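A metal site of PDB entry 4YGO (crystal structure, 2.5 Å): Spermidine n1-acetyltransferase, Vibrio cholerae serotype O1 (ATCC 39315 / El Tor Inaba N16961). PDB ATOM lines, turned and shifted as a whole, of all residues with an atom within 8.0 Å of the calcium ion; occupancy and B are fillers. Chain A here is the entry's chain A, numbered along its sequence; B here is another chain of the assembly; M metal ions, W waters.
Of the 20 residues printed, 3 come within 4 Å of the calcium ion.
The backbone carbonyl oxygen (O) of Asn 53 of chain B is in hydrogen-bond range of the side-chain hydroxyl (OH) of Tyr 78 of chain B (2.8 Å).
The backbone NH (N) of Glu 41 sits at hydrogen-bond distance from the side-chain hydroxyl (OG) of Ser 38 (3.1 Å).
OE1 of Glu 41 lies close to ND1 of His 51 of chain B, at 3.3 Å.
The calcium ion is bound by OE1 of Glu 41 (2.3 Å), O of Pro 35 (2.4 Å), OD1 of Asn 53 of chain B (2.5 Å) and water W1 (2.7 Å).
Slightly farther from the calcium ion lies OE2 of Glu 41 (3.0 Å).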
ATOM      1  N   MET A  28     -26.784  29.160  32.788  1.00  0.00           N
ATOM      2  CA  MET A  28     -26.569  28.913  31.371  1.00  0.00           C
ATOM      3  C   MET A  28     -27.682  28.018  30.879  1.00  0.00           C
ATOM      4  O   MET A  28     -28.052  27.079  31.561  1.00  0.00           O
ATOM      5  CB  MET A  28     -25.235  28.222  31.159  1.00  0.00           C
ATOM      6  CG  MET A  28     -24.894  27.878  29.712  1.00  0.00           C
ATOM      7  SD  MET A  28     -24.726  29.286  28.583  1.00  0.00           S
ATOM      8  CE  MET A  28     -23.125  29.908  29.141  1.00  0.00           C
ATOM      9  N   SER A  29     -28.192  28.259  29.695  1.00  0.00           N
ATOM     10  CA  SER A  29     -29.295  27.490  29.231  1.00  0.00           C
ATOM     11  C   SER A  29     -28.843  26.776  27.958  1.00  0.00           C
ATOM     12  O   SER A  29     -27.820  27.090  27.406  1.00  0.00           O
ATOM     13  CB  SER A  29     -30.569  28.363  29.090  1.00  0.00           C
ATOM     14  OG  SER A  29     -30.305  29.216  28.028  1.00  0.00           O
ATOM     15  N   GLU A  33     -28.420  20.138  24.443  1.00  0.00           N
ATOM     16  CA  GLU A  33     -27.121  20.011  25.122  1.00  0.00           C
ATOM     17  C   GLU A  33     -26.067  21.012  24.627  1.00  0.00           C
ATOM     18  O   GLU A  33     -24.963  21.047  25.182  1.00  0.00           O
ATOM     19  CB  GLU A  33     -26.640  18.537  25.202  1.00  0.00           C
ATOM     20  CG  GLU A  33     -27.766  17.702  25.829  1.00  0.00           C
ATOM     21  CD  GLU A  33     -27.384  16.299  26.266  1.00  0.00           C
ATOM     22  OE1 GLU A  33     -26.352  16.159  26.981  1.00  0.00           O
ATOM     23  OE2 GLU A  33     -28.174  15.359  25.946  1.00  0.00           O
ATOM     24  N   GLU A  34     -26.459  21.922  23.722  1.00  0.00           N
ATOM     25  CA  GLU A  34     -25.593  23.013  23.264  1.00  0.00           C
ATOM     26  C   GLU A  34     -25.919  24.228  24.129  1.00  0.00           C
ATOM     27  O   GLU A  34     -27.088  24.638  24.196  1.00  0.00           O
ATOM     28  CB  GLU A  34     -25.825  23.397  21.785  1.00  0.00           C
ATOM     29  CG  GLU A  34     -26.342  22.303  20.819  1.00  0.00           C
ATOM     30  CD  GLU A  34     -25.265  21.609  19.975  1.00  0.00           C
ATOM     31  OE1 GLU A  34     -24.087  21.552  20.450  1.00  0.00           O
ATOM     32  OE2 GLU A  34     -25.644  21.135  18.847  1.00  0.00           O
ATOM     33  N   PRO A  35     -24.905  24.798  24.777  1.00  0.00           N
ATOM     34  CA  PRO A  35     -25.100  26.078  25.443  1.00  0.00           C
ATOM     35  C   PRO A  35     -25.404  27.226  24.520  1.00  0.00           C
ATOM     36  O   PRO A  35     -24.823  27.309  23.416  1.00  0.00           O
ATOM     37  CB  PRO A  35     -23.737  26.340  26.142  1.00  0.00           C
ATOM     38  CG  PRO A  35     -22.792  25.435  25.480  1.00  0.00           C
ATOM     39  CD  PRO A  35     -23.594  24.224  25.116  1.00  0.00           C
ATOM     40  N   TYR A  36     -26.285  28.121  24.963  1.00  0.00           N
ATOM     41  CA  TYR A  36     -26.479  29.343  24.225  1.00  0.00           C
ATOM     42  C   TYR A  36     -26.802  30.511  25.106  1.00  0.00           C
ATOM     43  O   TYR A  36     -27.177  30.349  26.278  1.00  0.00           O
ATOM     44  CB  TYR A  36     -27.577  29.162  23.188  1.00  0.00           C
ATOM     45  CG  TYR A  36     -28.911  29.076  23.822  1.00  0.00           C
ATOM     46  CD1 TYR A  36     -29.351  27.884  24.369  1.00  0.00           C
ATOM     47  CD2 TYR A  36     -29.710  30.194  23.914  1.00  0.00           C
ATOM     48  CE1 TYR A  36     -30.589  27.822  24.979  1.00  0.00           C
ATOM     49  CE2 TYR A  36     -30.909  30.155  24.546  1.00  0.00           C
ATOM     50  CZ  TYR A  36     -31.352  28.975  25.078  1.00  0.00           C
ATOM     51  OH  TYR A  36     -32.581  28.947  25.699  1.00  0.00           O
ATOM     52  N   GLU A  37     -26.640  31.707  24.523  1.00  0.00           N
ATOM     53  CA  GLU A  37     -26.962  32.975  25.202  1.00  0.00           C
ATOM     54  C   GLU A  37     -27.776  33.932  24.343  1.00  0.00           C
ATOM     55  O   GLU A  37     -28.646  34.607  24.887  1.00  0.00           O
ATOM     56  CB  GLU A  37     -25.672  33.670  25.668  1.00  0.00           C
ATOM     57  CG  GLU A  37     -24.839  32.684  26.465  1.00  0.00           C
ATOM     58  CD  GLU A  37     -23.560  33.189  26.932  1.00  0.00           C
ATOM     59  OE1 GLU A  37     -23.362  33.066  28.144  1.00  0.00           O
ATOM     60  OE2 GLU A  37     -22.760  33.641  26.133  1.00  0.00           O
ATOM     61  N   SER A  38     -27.442  34.049  23.058  1.00  0.00           N
ATOM     62  CA  SER A  38     -28.142  34.933  22.150  1.00  0.00           C
ATOM     63  C   SER A  38     -29.343  34.217  21.491  1.00  0.00           C
ATOM     64  O   SER A  38     -29.314  32.995  21.247  1.00  0.00           O
ATOM     65  CB  SER A  38     -27.205  35.435  21.064  1.00  0.00           C
ATOM     66  OG  SER A  38     -26.785  34.400  20.212  1.00  0.00           O
ATOM     67  N   GLU A  41     -28.232  32.490  18.317  1.00  0.00           N
ATOM     68  CA  GLU A  41     -27.728  31.131  18.414  1.00  0.00           C
ATOM     69  C   GLU A  41     -28.859  30.143  18.707  1.00  0.00           C
ATOM     70  O   GLU A  41     -28.889  29.044  18.163  1.00  0.00           O
ATOM     71  CB  GLU A  41     -26.607  31.029  19.442  1.00  0.00           C
ATOM     72  CG  GLU A  41     -25.742  29.804  19.185  1.00  0.00           C
ATOM     73  CD  GLU A  41     -24.816  29.457  20.319  1.00  0.00           C
ATOM     74  OE1 GLU A  41     -24.303  28.295  20.308  1.00  0.00           O
ATOM     75  OE2 GLU A  41     -24.585  30.371  21.192  1.00  0.00           O
ATOM     76  N   LEU A  42     -29.770  30.538  19.579  1.00  0.00           N
ATOM     77  CA  LEU A  42     -30.961  29.803  19.829  1.00  0.00           C
ATOM     78  C   LEU A  42     -31.734  29.460  18.541  1.00  0.00           C
ATOM     79  O   LEU A  42     -32.089  28.269  18.275  1.00  0.00           O
ATOM     80  CB  LEU A  42     -31.861  30.602  20.793  1.00  0.00           C
ATOM     81  CG  LEU A  42     -33.233  29.952  21.037  1.00  0.00           C
ATOM     82  CD1 LEU A  42     -33.043  28.587  21.659  1.00  0.00           C
ATOM     83  CD2 LEU A  42     -34.170  30.775  21.912  1.00  0.00           C
ATOM     84  N   LEU A  45     -29.921  26.858  16.630  1.00  0.00           N
ATOM     85  CA  LEU A  45     -30.080  25.564  17.266  1.00  0.00           C
ATOM     86  C   LEU A  45     -31.479  24.987  17.056  1.00  0.00           C
ATOM     87  O   LEU A  45     -31.618  23.804  16.794  1.00  0.00           O
ATOM     88  CB  LEU A  45     -29.814  25.676  18.725  1.00  0.00           C
ATOM     89  CG  LEU A  45     -28.438  25.361  19.340  1.00  0.00           C
ATOM     90  CD1 LEU A  45     -27.354  24.922  18.380  1.00  0.00           C
ATOM     91  CD2 LEU A  45     -28.026  26.565  20.155  1.00  0.00           C
ATOM     92  N   HIS B  49     -19.152  31.901  13.143  1.00  0.00           N
ATOM     93  CA  HIS B  49     -18.643  31.503  14.475  1.00  0.00           C
ATOM     94  C   HIS B  49     -19.687  31.503  15.558  1.00  0.00           C
ATOM     95  O   HIS B  49     -19.379  31.404  16.743  1.00  0.00           O
ATOM     96  CB  HIS B  49     -17.495  32.417  14.875  1.00  0.00           C
ATOM     97  CG  HIS B  49     -16.235  32.140  14.127  1.00  0.00           C
ATOM     98  ND1 HIS B  49     -15.313  31.204  14.558  1.00  0.00           N
ATOM     99  CD2 HIS B  49     -15.718  32.690  13.012  1.00  0.00           C
ATOM    100  CE1 HIS B  49     -14.301  31.162  13.712  1.00  0.00           C
ATOM    101  NE2 HIS B  49     -14.532  32.050  12.775  1.00  0.00           N
ATOM    102  N   ILE B  50     -20.931  31.506  15.155  1.00  0.00           N
ATOM    103  CA  ILE B  50     -22.008  31.605  16.091  1.00  0.00           C
ATOM    104  C   ILE B  50     -22.062  30.471  17.062  1.00  0.00           C
ATOM    105  O   ILE B  50     -22.518  30.689  18.200  1.00  0.00           O
ATOM    106  CB  ILE B  50     -23.340  31.778  15.302  1.00  0.00           C
ATOM    107  CG1 ILE B  50     -24.426  32.437  16.135  1.00  0.00           C
ATOM    108  CG2 ILE B  50     -23.817  30.491  14.650  1.00  0.00           C
ATOM    109  CD1 ILE B  50     -25.329  33.198  15.248  1.00  0.00           C
ATOM    110  N   HIS B  51     -21.633  29.259  16.680  1.00  0.00           N
ATOM    111  CA  HIS B  51     -21.559  28.179  17.692  1.00  0.00           C
ATOM    112  C   HIS B  51     -20.201  28.024  18.377  1.00  0.00           C
ATOM    113  O   HIS B  51     -20.053  27.130  19.199  1.00  0.00           O
ATOM    114  CB  HIS B  51     -21.997  26.828  17.136  1.00  0.00           C
ATOM    115  CG  HIS B  51     -23.358  26.855  16.509  1.00  0.00           C
ATOM    116  ND1 HIS B  51     -24.483  27.284  17.181  1.00  0.00           N
ATOM    117  CD2 HIS B  51     -23.759  26.537  15.262  1.00  0.00           C
ATOM    118  CE1 HIS B  51     -25.514  27.211  16.374  1.00  0.00           C
ATOM    119  NE2 HIS B  51     -25.105  26.779  15.201  1.00  0.00           N
ATOM    120  N   ASP B  52     -19.242  28.878  18.080  1.00  0.00           N
ATOM    121  CA  ASP B  52     -17.927  28.805  18.644  1.00  0.00           C
ATOM    122  C   ASP B  52     -18.008  29.406  20.032  1.00  0.00           C
ATOM    123  O   ASP B  52     -18.363  30.556  20.206  1.00  0.00           O
ATOM    124  CB  ASP B  52     -16.946  29.537  17.742  1.00  0.00           C
ATOM    125  CG  ASP B  52     -15.473  29.173  17.992  1.00  0.00           C
ATOM    126  OD1 ASP B  52     -15.081  28.793  19.108  1.00  0.00           O
ATOM    127  OD2 ASP B  52     -14.664  29.338  17.021  1.00  0.00           O
ATOM    128  N   ASN B  53     -17.659  28.593  21.028  1.00  0.00           N
ATOM    129  CA  ASN B  53     -17.666  29.010  22.418  1.00  0.00           C
ATOM    130  C   ASN B  53     -16.313  29.537  22.988  1.00  0.00           C
ATOM    131  O   ASN B  53     -16.205  29.824  24.202  1.00  0.00           O
ATOM    132  CB  ASN B  53     -18.279  27.878  23.264  1.00  0.00           C
ATOM    133  CG  ASN B  53     -19.764  27.624  22.905  1.00  0.00           C
ATOM    134  OD1 ASN B  53     -20.580  28.553  22.799  1.00  0.00           O
ATOM    135  ND2 ASN B  53     -20.117  26.335  22.729  1.00  0.00           N
ATOM    136  N   ALA B  54     -15.335  29.703  22.125  1.00  0.00           N
ATOM    137  CA  ALA B  54     -14.040  30.306  22.523  1.00  0.00           C
ATOM    138  C   ALA B  54     -14.072  31.840  22.769  1.00  0.00           C
ATOM    139  O   ALA B  54     -13.132  32.399  23.360  1.00  0.00           O
ATOM    140  CB  ALA B  54     -12.975  29.989  21.505  1.00  0.00           C
ATOM    141  N   GLU B  55     -15.110  32.498  22.269  1.00  0.00           N
ATOM    142  CA  GLU B  55     -15.318  33.915  22.524  1.00  0.00           C
ATOM    143  C   GLU B  55     -16.787  34.148  22.802  1.00  0.00           C
ATOM    144  O   GLU B  55     -17.684  33.451  22.241  1.00  0.00           O
ATOM    145  CB  GLU B  55     -14.825  34.789  21.337  1.00  0.00           C
ATOM    146  CG  GLU B  55     -13.449  34.378  20.833  1.00  0.00           C
ATOM    147  CD  GLU B  55     -12.807  35.304  19.807  1.00  0.00           C
ATOM    148  OE1 GLU B  55     -11.548  35.212  19.656  1.00  0.00           O
ATOM    149  OE2 GLU B  55     -13.519  36.059  19.120  1.00  0.00           O
ATOM    150  N   ARG B  56     -17.041  35.086  23.691  1.00  0.00           N
ATOM    151  CA  ARG B  56     -18.397  35.510  24.013  1.00  0.00           C
ATOM    152  C   ARG B  56     -18.421  37.021  24.217  1.00  0.00           C
ATOM    153  O   ARG B  56     -17.568  37.584  24.888  1.00  0.00           O
ATOM    154  CB  ARG B  56     -18.906  34.820  25.250  1.00  0.00           C
ATOM    155  CG  ARG B  56     -18.956  33.337  25.117  1.00  0.00           C
ATOM    156  CD  ARG B  56     -19.610  32.756  26.346  1.00  0.00           C
ATOM    157  NE  ARG B  56     -19.571  31.283  26.442  1.00  0.00           N
ATOM    158  CZ  ARG B  56     -20.560  30.439  26.140  1.00  0.00           C
ATOM    159  NH1 ARG B  56     -21.745  30.853  25.688  1.00  0.00           N
ATOM    160  NH2 ARG B  56     -20.327  29.129  26.296  1.00  0.00           N
ATOM    161  N   TYR B  78     -11.784  25.762  28.400  1.00  0.00           N
ATOM    162  CA  TYR B  78     -12.550  25.118  29.428  1.00  0.00           C
ATOM    163  C   TYR B  78     -11.851  23.987  30.144  1.00  0.00           C
ATOM    164  O   TYR B  78     -12.471  23.317  30.977  1.00  0.00           O
ATOM    165  CB  TYR B  78     -13.895  24.648  28.824  1.00  0.00           C
ATOM    166  CG  TYR B  78     -14.757  25.816  28.289  1.00  0.00           C
ATOM    167  CD1 TYR B  78     -15.572  26.599  29.164  1.00  0.00           C
ATOM    168  CD2 TYR B  78     -14.769  26.132  26.922  1.00  0.00           C
ATOM    169  CE1 TYR B  78     -16.377  27.641  28.664  1.00  0.00           C
ATOM    170  CE2 TYR B  78     -15.538  27.197  26.421  1.00  0.00           C
ATOM    171  CZ  TYR B  78     -16.348  27.946  27.282  1.00  0.00           C
ATOM    172  OH  TYR B  78     -17.125  28.994  26.732  1.00  0.00           O
HETATM  173 CA    CA M   1     -22.974  28.086  22.182  1.00  0.00          CA
HETATM  174  O   HOH W   1     -23.009  25.551  21.394  1.00  0.00           O
